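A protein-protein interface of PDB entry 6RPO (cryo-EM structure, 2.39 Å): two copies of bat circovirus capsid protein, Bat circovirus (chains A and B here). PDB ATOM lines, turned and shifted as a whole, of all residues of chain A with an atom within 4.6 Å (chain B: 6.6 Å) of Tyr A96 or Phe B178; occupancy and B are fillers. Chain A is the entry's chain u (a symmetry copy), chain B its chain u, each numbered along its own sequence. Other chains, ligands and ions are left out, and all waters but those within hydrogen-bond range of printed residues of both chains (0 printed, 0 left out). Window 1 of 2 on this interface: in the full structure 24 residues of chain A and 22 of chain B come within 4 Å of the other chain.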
ATOM      1  N   PHE A  94      11.495 -37.394  17.581  1.00  0.00           N
ATOM      2  CA  PHE A  94      10.502 -36.365  17.812  1.00  0.00           C
ATOM      3  C   PHE A  94      10.927 -35.100  17.093  1.00  0.00           C
ATOM      4  O   PHE A  94      12.111 -34.779  17.003  1.00  0.00           O
ATOM      5  CB  PHE A  94      10.300 -36.098  19.305  1.00  0.00           C
ATOM      6  CG  PHE A  94       9.785 -37.280  20.043  1.00  0.00           C
ATOM      7  CD1 PHE A  94       8.447 -37.625  19.961  1.00  0.00           C
ATOM      8  CD2 PHE A  94      10.643 -38.080  20.777  1.00  0.00           C
ATOM      9  CE1 PHE A  94       7.969 -38.729  20.617  1.00  0.00           C
ATOM     10  CE2 PHE A  94      10.167 -39.187  21.436  1.00  0.00           C
ATOM     11  CZ  PHE A  94       8.827 -39.511  21.353  1.00  0.00           C
ATOM     12  N   LYS A  95       9.935 -34.382  16.585  1.00  0.00           N
ATOM     13  CA  LYS A  95      10.159 -33.190  15.784  1.00  0.00           C
ATOM     14  C   LYS A  95      10.403 -31.933  16.609  1.00  0.00           C
ATOM     15  O   LYS A  95      11.184 -31.079  16.191  1.00  0.00           O
ATOM     16  CB  LYS A  95       8.960 -32.970  14.858  1.00  0.00           C
ATOM     17  CG  LYS A  95       9.310 -32.429  13.504  1.00  0.00           C
ATOM     18  CD  LYS A  95       8.141 -32.554  12.559  1.00  0.00           C
ATOM     19  CE  LYS A  95       8.515 -32.075  11.175  1.00  0.00           C
ATOM     20  NZ  LYS A  95       9.032 -30.689  11.210  1.00  0.00           N
ATOM     21  N   TYR A  96       9.751 -31.781  17.759  1.00  0.00           N
ATOM     22  CA  TYR A  96       9.831 -30.562  18.551  1.00  0.00           C
ATOM     23  C   TYR A  96      10.117 -30.886  20.011  1.00  0.00           C
ATOM     24  O   TYR A  96       9.902 -32.006  20.473  1.00  0.00           O
ATOM     25  CB  TYR A  96       8.541 -29.738  18.461  1.00  0.00           C
ATOM     26  CG  TYR A  96       7.989 -29.614  17.069  1.00  0.00           C
ATOM     27  CD1 TYR A  96       8.653 -28.875  16.102  1.00  0.00           C
ATOM     28  CD2 TYR A  96       6.811 -30.249  16.718  1.00  0.00           C
ATOM     29  CE1 TYR A  96       8.156 -28.771  14.828  1.00  0.00           C
ATOM     30  CE2 TYR A  96       6.301 -30.146  15.452  1.00  0.00           C
ATOM     31  CZ  TYR A  96       6.975 -29.408  14.511  1.00  0.00           C
ATOM     32  OH  TYR A  96       6.459 -29.315  13.247  1.00  0.00           O
ATOM     33  N   TYR A  97      10.620 -29.887  20.732  1.00  0.00           N
ATOM     34  CA  TYR A  97      10.918 -30.044  22.148  1.00  0.00           C
ATOM     35  C   TYR A  97      10.845 -28.695  22.844  1.00  0.00           C
ATOM     36  O   TYR A  97      10.921 -27.642  22.215  1.00  0.00           O
ATOM     37  CB  TYR A  97      12.301 -30.677  22.383  1.00  0.00           C
ATOM     38  CG  TYR A  97      13.456 -29.724  22.196  1.00  0.00           C
ATOM     39  CD1 TYR A  97      13.899 -29.391  20.928  1.00  0.00           C
ATOM     40  CD2 TYR A  97      14.106 -29.157  23.293  1.00  0.00           C
ATOM     41  CE1 TYR A  97      14.938 -28.523  20.750  1.00  0.00           C
ATOM     42  CE2 TYR A  97      15.143 -28.278  23.122  1.00  0.00           C
ATOM     43  CZ  TYR A  97      15.560 -27.974  21.849  1.00  0.00           C
ATOM     44  OH  TYR A  97      16.602 -27.107  21.667  1.00  0.00           O
ATOM     45  N   LEU A 187       7.574 -21.568  24.714  1.00  0.00           N
ATOM     46  CA  LEU A 187       7.789 -21.724  23.278  1.00  0.00           C
ATOM     47  C   LEU A 187       8.340 -23.100  22.911  1.00  0.00           C
ATOM     48  O   LEU A 187       9.090 -23.713  23.671  1.00  0.00           O
ATOM     49  CB  LEU A 187       8.745 -20.645  22.776  1.00  0.00           C
ATOM     50  CG  LEU A 187       8.249 -19.202  22.819  1.00  0.00           C
ATOM     51  CD1 LEU A 187       9.424 -18.250  22.823  1.00  0.00           C
ATOM     52  CD2 LEU A 187       7.312 -18.904  21.663  1.00  0.00           C
ATOM     53  N   TRP A 188       7.963 -23.576  21.727  1.00  0.00           N
ATOM     54  CA  TRP A 188       8.438 -24.836  21.169  1.00  0.00           C
ATOM     55  C   TRP A 188       9.565 -24.587  20.177  1.00  0.00           C
ATOM     56  O   TRP A 188       9.612 -23.558  19.501  1.00  0.00           O
ATOM     57  CB  TRP A 188       7.319 -25.599  20.462  1.00  0.00           C
ATOM     58  CG  TRP A 188       6.294 -26.237  21.344  1.00  0.00           C
ATOM     59  CD1 TRP A 188       5.048 -25.768  21.615  1.00  0.00           C
ATOM     60  CD2 TRP A 188       6.409 -27.489  22.036  1.00  0.00           C
ATOM     61  NE1 TRP A 188       4.387 -26.630  22.446  1.00  0.00           N
ATOM     62  CE2 TRP A 188       5.196 -27.700  22.712  1.00  0.00           C
ATOM     63  CE3 TRP A 188       7.419 -28.447  22.149  1.00  0.00           C
ATOM     64  CZ2 TRP A 188       4.969 -28.824  23.498  1.00  0.00           C
ATOM     65  CZ3 TRP A 188       7.192 -29.558  22.925  1.00  0.00           C
ATOM     66  CH2 TRP A 188       5.976 -29.740  23.588  1.00  0.00           C
ATOM     67  N   PHE A 189      10.477 -25.547  20.094  1.00  0.00           N
ATOM     68  CA  PHE A 189      11.646 -25.424  19.243  1.00  0.00           C
ATOM     69  C   PHE A 189      11.843 -26.702  18.443  1.00  0.00           C
ATOM     70  O   PHE A 189      11.559 -27.791  18.945  1.00  0.00           O
ATOM     71  CB  PHE A 189      12.897 -25.126  20.085  1.00  0.00           C
ATOM     72  CG  PHE A 189      12.886 -23.761  20.692  1.00  0.00           C
ATOM     73  CD1 PHE A 189      13.425 -22.690  20.008  1.00  0.00           C
ATOM     74  CD2 PHE A 189      12.297 -23.537  21.931  1.00  0.00           C
ATOM     75  CE1 PHE A 189      13.405 -21.431  20.553  1.00  0.00           C
ATOM     76  CE2 PHE A 189      12.268 -22.280  22.472  1.00  0.00           C
ATOM     77  CZ  PHE A 189      12.826 -21.226  21.778  1.00  0.00           C
ATOM     78  N   PRO A 190      12.317 -26.606  17.201  1.00  0.00           N
ATOM     79  CA  PRO A 190      12.598 -27.820  16.424  1.00  0.00           C
ATOM     80  C   PRO A 190      13.845 -28.523  16.934  1.00  0.00           C
ATOM     81  O   PRO A 190      14.847 -27.882  17.257  1.00  0.00           O
ATOM     82  CB  PRO A 190      12.802 -27.296  14.995  1.00  0.00           C
ATOM     83  CG  PRO A 190      12.451 -25.864  15.025  1.00  0.00           C
ATOM     84  CD  PRO A 190      12.552 -25.386  16.419  1.00  0.00           C
ATOM     85  N   ASN A 191      13.768 -29.845  17.013  1.00  0.00           N
ATOM     86  CA  ASN A 191      14.912 -30.687  17.336  1.00  0.00           C
ATOM     87  C   ASN A 191      15.646 -31.001  16.036  1.00  0.00           C
ATOM     88  O   ASN A 191      15.161 -31.786  15.217  1.00  0.00           O
ATOM     89  CB  ASN A 191      14.434 -31.952  18.046  1.00  0.00           C
ATOM     90  CG  ASN A 191      15.526 -32.989  18.217  1.00  0.00           C
ATOM     91  OD1 ASN A 191      16.691 -32.663  18.438  1.00  0.00           O
ATOM     92  ND2 ASN A 191      15.149 -34.250  18.115  1.00  0.00           N
ATOM     93  N   GLN A 224      10.336 -32.071  27.372  1.00  0.00           N
ATOM     94  CA  GLN A 224       9.039 -32.463  26.842  1.00  0.00           C
ATOM     95  C   GLN A 224       9.124 -32.452  25.322  1.00  0.00           C
ATOM     96  O   GLN A 224       9.417 -31.415  24.729  1.00  0.00           O
ATOM     97  CB  GLN A 224       7.947 -31.525  27.356  1.00  0.00           C
ATOM     98  CG  GLN A 224       6.584 -31.710  26.742  1.00  0.00           C
ATOM     99  CD  GLN A 224       5.487 -31.054  27.559  1.00  0.00           C
ATOM    100  OE1 GLN A 224       5.064 -31.573  28.587  1.00  0.00           O
ATOM    101  NE2 GLN A 224       5.032 -29.903  27.109  1.00  0.00           N
ATOM    102  N   PHE A 225       8.891 -33.600  24.697  1.00  0.00           N
ATOM    103  CA  PHE A 225       8.975 -33.750  23.249  1.00  0.00           C
ATOM    104  C   PHE A 225       7.586 -33.791  22.621  1.00  0.00           C
ATOM    105  O   PHE A 225       6.590 -34.098  23.275  1.00  0.00           O
ATOM    106  CB  PHE A 225       9.747 -35.016  22.874  1.00  0.00           C
ATOM    107  CG  PHE A 225      11.226 -34.902  23.039  1.00  0.00           C
ATOM    108  CD1 PHE A 225      11.994 -34.259  22.087  1.00  0.00           C
ATOM    109  CD2 PHE A 225      11.855 -35.463  24.136  1.00  0.00           C
ATOM    110  CE1 PHE A 225      13.359 -34.165  22.233  1.00  0.00           C
ATOM    111  CE2 PHE A 225      13.218 -35.375  24.287  1.00  0.00           C
ATOM    112  CZ  PHE A 225      13.973 -34.721  23.335  1.00  0.00           C
ATOM    113  N   ARG A 226       7.536 -33.501  21.321  1.00  0.00           N
ATOM    114  CA  ARG A 226       6.283 -33.419  20.581  1.00  0.00           C
ATOM    115  C   ARG A 226       6.515 -33.899  19.150  1.00  0.00           C
ATOM    116  O   ARG A 226       7.619 -33.751  18.626  1.00  0.00           O
ATOM    117  CB  ARG A 226       5.748 -31.977  20.607  1.00  0.00           C
ATOM    118  CG  ARG A 226       4.385 -31.749  19.978  1.00  0.00           C
ATOM    119  CD  ARG A 226       3.957 -30.308  20.079  1.00  0.00           C
ATOM    120  NE  ARG A 226       2.896 -30.004  19.129  1.00  0.00           N
ATOM    121  CZ  ARG A 226       2.213 -28.867  19.115  1.00  0.00           C
ATOM    122  NH1 ARG A 226       1.270 -28.673  18.212  1.00  0.00           N
ATOM    123  NH2 ARG A 226       2.471 -27.928  20.007  1.00  0.00           N
ATOM    124  N   GLU A 227       5.466 -34.471  18.534  1.00  0.00           N
ATOM    125  CA  GLU A 227       5.401 -34.876  17.120  1.00  0.00           C
ATOM    126  C   GLU A 227       6.437 -35.960  16.785  1.00  0.00           C
ATOM    127  O   GLU A 227       7.521 -35.707  16.260  1.00  0.00           O
ATOM    128  CB  GLU A 227       5.514 -33.672  16.173  1.00  0.00           C
ATOM    129  CG  GLU A 227       5.309 -33.990  14.683  1.00  0.00           C
ATOM    130  CD  GLU A 227       4.075 -34.837  14.393  1.00  0.00           C
ATOM    131  OE1 GLU A 227       2.957 -34.280  14.332  1.00  0.00           O
ATOM    132  OE2 GLU A 227       4.224 -36.060  14.211  1.00  0.00           O
ATOM    133  N   PRO B 124       0.207 -31.505   9.172  1.00  0.00           N
ATOM    134  CA  PRO B 124       0.565 -30.123   9.517  1.00  0.00           C
ATOM    135  C   PRO B 124       1.996 -30.064  10.030  1.00  0.00           C
ATOM    136  O   PRO B 124       2.396 -30.851  10.891  1.00  0.00           O
ATOM    137  CB  PRO B 124      -0.456 -29.758  10.605  1.00  0.00           C
ATOM    138  CG  PRO B 124      -1.519 -30.818  10.523  1.00  0.00           C
ATOM    139  CD  PRO B 124      -0.816 -32.045  10.076  1.00  0.00           C
ATOM    140  N   ILE B 125       2.777 -29.146   9.484  1.00  0.00           N
ATOM    141  CA  ILE B 125       4.176 -28.982   9.852  1.00  0.00           C
ATOM    142  C   ILE B 125       4.349 -27.525  10.259  1.00  0.00           C
ATOM    143  O   ILE B 125       4.212 -26.612   9.443  1.00  0.00           O
ATOM    144  CB  ILE B 125       5.114 -29.408   8.720  1.00  0.00           C
ATOM    145  CG1 ILE B 125       5.079 -30.935   8.591  1.00  0.00           C
ATOM    146  CG2 ILE B 125       6.535 -28.934   8.982  1.00  0.00           C
ATOM    147  CD1 ILE B 125       5.856 -31.507   7.471  1.00  0.00           C
ATOM    148  N   LEU B 126       4.624 -27.309  11.542  1.00  0.00           N
ATOM    149  CA  LEU B 126       4.534 -25.983  12.130  1.00  0.00           C
ATOM    150  C   LEU B 126       5.842 -25.205  12.111  1.00  0.00           C
ATOM    151  O   LEU B 126       5.810 -23.983  12.269  1.00  0.00           O
ATOM    152  CB  LEU B 126       4.024 -26.082  13.570  1.00  0.00           C
ATOM    153  CG  LEU B 126       2.666 -26.772  13.733  1.00  0.00           C
ATOM    154  CD1 LEU B 126       2.224 -26.770  15.181  1.00  0.00           C
ATOM    155  CD2 LEU B 126       1.612 -26.117  12.853  1.00  0.00           C
ATOM    156  N   ASP B 127       6.985 -25.868  11.938  1.00  0.00           N
ATOM    157  CA  ASP B 127       8.251 -25.145  11.938  1.00  0.00           C
ATOM    158  C   ASP B 127       8.729 -24.790  10.534  1.00  0.00           C
ATOM    159  O   ASP B 127       9.776 -24.152  10.394  1.00  0.00           O
ATOM    160  CB  ASP B 127       9.331 -25.951  12.666  1.00  0.00           C
ATOM    161  CG  ASP B 127       9.633 -27.291  11.998  1.00  0.00           C
ATOM    162  OD1 ASP B 127       8.829 -27.769  11.173  1.00  0.00           O
ATOM    163  OD2 ASP B 127      10.694 -27.869  12.299  1.00  0.00           O
ATOM    164  N   GLY B 128       8.007 -25.208   9.501  1.00  0.00           N
ATOM    165  CA  GLY B 128       8.428 -24.970   8.142  1.00  0.00           C
ATOM    166  C   GLY B 128       9.538 -25.871   7.643  1.00  0.00           C
ATOM    167  O   GLY B 128      10.195 -25.520   6.659  1.00  0.00           O
ATOM    168  N   ALA B 129       9.772 -27.013   8.285  1.00  0.00           N
ATOM    169  CA  ALA B 129      10.813 -27.950   7.879  1.00  0.00           C
ATOM    170  C   ALA B 129      10.156 -29.211   7.331  1.00  0.00           C
ATOM    171  O   ALA B 129       9.673 -30.048   8.097  1.00  0.00           O
ATOM    172  CB  ALA B 129      11.738 -28.275   9.047  1.00  0.00           C
ATOM    173  N   LYS B 168       1.411 -21.570  12.189  1.00  0.00           N
ATOM    174  CA  LYS B 168       2.388 -20.844  12.971  1.00  0.00           C
ATOM    175  C   LYS B 168       3.225 -19.948  12.067  1.00  0.00           C
ATOM    176  O   LYS B 168       3.592 -20.364  10.961  1.00  0.00           O
ATOM    177  CB  LYS B 168       3.291 -21.808  13.754  1.00  0.00           C
ATOM    178  CG  LYS B 168       2.523 -22.780  14.606  1.00  0.00           C
ATOM    179  CD  LYS B 168       1.853 -22.062  15.763  1.00  0.00           C
ATOM    180  CE  LYS B 168       0.760 -22.901  16.383  1.00  0.00           C
ATOM    181  NZ  LYS B 168       0.262 -22.291  17.642  1.00  0.00           N
ATOM    182  N   PRO B 169       3.526 -18.722  12.484  1.00  0.00           N
ATOM    183  CA  PRO B 169       4.321 -17.823  11.642  1.00  0.00           C
ATOM    184  C   PRO B 169       5.793 -18.200  11.630  1.00  0.00           C
ATOM    185  O   PRO B 169       6.345 -18.680  12.621  1.00  0.00           O
ATOM    186  CB  PRO B 169       4.108 -16.456  12.302  1.00  0.00           C
ATOM    187  CG  PRO B 169       3.804 -16.777  13.718  1.00  0.00           C
ATOM    188  CD  PRO B 169       3.048 -18.061  13.709  1.00  0.00           C
ATOM    189  N   GLY B 176      13.751 -20.931  15.022  1.00  0.00           N
ATOM    190  CA  GLY B 176      12.532 -21.561  14.535  1.00  0.00           C
ATOM    191  C   GLY B 176      11.467 -21.776  15.589  1.00  0.00           C
ATOM    192  O   GLY B 176      10.701 -22.740  15.498  1.00  0.00           O
ATOM    193  N   PHE B 177      11.402 -20.899  16.585  1.00  0.00           N
ATOM    194  CA  PHE B 177      10.456 -21.048  17.681  1.00  0.00           C
ATOM    195  C   PHE B 177       9.024 -20.787  17.222  1.00  0.00           C
ATOM    196  O   PHE B 177       8.780 -20.070  16.249  1.00  0.00           O
ATOM    197  CB  PHE B 177      10.820 -20.106  18.834  1.00  0.00           C
ATOM    198  CG  PHE B 177      10.609 -18.638  18.537  1.00  0.00           C
ATOM    199  CD1 PHE B 177      11.579 -17.907  17.879  1.00  0.00           C
ATOM    200  CD2 PHE B 177       9.459 -17.981  18.957  1.00  0.00           C
ATOM    201  CE1 PHE B 177      11.398 -16.572  17.620  1.00  0.00           C
ATOM    202  CE2 PHE B 177       9.273 -16.646  18.691  1.00  0.00           C
ATOM    203  CZ  PHE B 177      10.247 -15.940  18.028  1.00  0.00           C
ATOM    204  N   PHE B 178       8.070 -21.375  17.941  1.00  0.00           N
ATOM    205  CA  PHE B 178       6.657 -21.090  17.726  1.00  0.00           C
ATOM    206  C   PHE B 178       5.897 -21.272  19.033  1.00  0.00           C
ATOM    207  O   PHE B 178       6.291 -22.042  19.907  1.00  0.00           O
ATOM    208  CB  PHE B 178       6.046 -21.960  16.599  1.00  0.00           C
ATOM    209  CG  PHE B 178       6.048 -23.447  16.870  1.00  0.00           C
ATOM    210  CD1 PHE B 178       7.146 -24.224  16.536  1.00  0.00           C
ATOM    211  CD2 PHE B 178       4.932 -24.077  17.402  1.00  0.00           C
ATOM    212  CE1 PHE B 178       7.145 -25.590  16.763  1.00  0.00           C
ATOM    213  CE2 PHE B 178       4.930 -25.441  17.639  1.00  0.00           C
ATOM    214  CZ  PHE B 178       6.039 -26.199  17.319  1.00  0.00           C
ATOM    215  N   GLN B 179       4.801 -20.568  19.142  1.00  0.00           N
ATOM    216  CA  GLN B 179       3.933 -20.527  20.305  1.00  0.00           C
ATOM    217  C   GLN B 179       3.091 -21.789  20.401  1.00  0.00           C
ATOM    218  O   GLN B 179       2.815 -22.445  19.396  1.00  0.00           O
ATOM    219  CB  GLN B 179       3.007 -19.305  20.235  1.00  0.00           C
ATOM    220  CG  GLN B 179       3.659 -17.994  20.613  1.00  0.00           C
ATOM    221  CD  GLN B 179       2.673 -16.844  20.697  1.00  0.00           C
ATOM    222  OE1 GLN B 179       2.549 -16.198  21.733  1.00  0.00           O
ATOM    223  NE2 GLN B 179       1.988 -16.567  19.601  1.00  0.00           N
ATOM    224  N   PRO B 180       2.680 -22.174  21.607  1.00  0.00           N
ATOM    225  CA  PRO B 180       1.583 -23.137  21.737  1.00  0.00           C
ATOM    226  C   PRO B 180       0.257 -22.498  21.347  1.00  0.00           C
ATOM    227  O   PRO B 180       0.135 -21.287  21.179  1.00  0.00           O
ATOM    228  CB  PRO B 180       1.604 -23.518  23.221  1.00  0.00           C
ATOM    229  CG  PRO B 180       2.886 -23.019  23.749  1.00  0.00           C
ATOM    230  CD  PRO B 180       3.306 -21.877  22.903  1.00  0.00           C
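The backbone carbonyl oxygen (O) of Ala B129 is in hydrogen-bond range of the side-chain amino group (NZ) of Lys A95, at 3.2 Å.
The backbone NH (N) of Leu B126 lies within hydrogen-bond range of the side-chain hydroxyl (OH) of Tyr A96, 3.2 Å away.
OD1 of Asp B127 lies within salt-bridge range of NZ of Lys A95, at 2.9 Å.
O of Phe B178 sits at hydrogen-bond distance from N of Trp A188 (2.9 Å).
N of Ala B129 sits at hydrogen-bond distance from OD1 of Asp B127, at 3.1 Å.
O of Lys A95 sits at hydrogen-bond distance from N of Asn A191.
NZ of Lys B168 is in hydrogen-bond range of O of Gln B179 (3.1 Å).
The backbone carbonyl oxygen of Arg A226 lies within hydrogen-bond range of the backbone NH of Lys A95.
N of Arg A226 is in hydrogen-bond range of O of Tyr A96, at 2.9 Å.
O of Phe A189 sits at hydrogen-bond distance from N of Tyr A97 (2.9 Å).
Among the printed residues, merely in contact across the chains: Lys A95 with Ile B125 (3.8 Å), Tyr A96 with Asp B127 (3.5 Å), Tyr A96 with Phe B178 (3.7 Å), Leu A187 with Phe B177 (3.6 Å), Leu A187 with Phe B178 (3.7 Å), Leu A187 with Gln B179 (3.9 Å), Trp A188 with Phe B177 (3.2 Å), Phe A189 with Phe B177 (3.4 Å), Pro A190 with Asp B127 (3.5 Å), Pro A190 with Gly B176 (3.4 Å) and Arg A226 with Leu B126 (3.7 Å).
Tyr A96 touches three residues of chain B.
Asn A191 touches none of the printed residues of chain B.
Of the printed residues of chain B, Arg A226 touches Leu B126.
Glu A227 touches none of the printed residues of chain B.
Of the printed residues of chain A, Ile B125 touches Lys A95 (3.8 Å).
Printed residues of chain A within 4 Å of Gly B176: Pro A190 (3.4 Å).
Phe B178 touches three residues of chain A.
Of the printed residues of chain A, Gln B179 touches Leu A187.
The nearest residue of chain A that does not touch Phe B178 is Arg A226 (4.2 Å).
The nearest printed residue of chain A that does not touch Ile B125 is Tyr A96 (4.1 Å).
Of the 13 printed residues of chain A, 7 touch a printed residue of chain B.
Along chain A the printed residues that touch a printed residue of chain B span positions 95 to 226.
Of the 13 printed residues of chain B, 8 touch a printed residue of chain A.
Along chain B the printed residues that touch a printed residue of chain A span positions 125 to 179.
No position is printed for both chains.
Of the 15 pairs that touch across the chains among the printed residues, none has its exchanged pair printed and touching as well.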
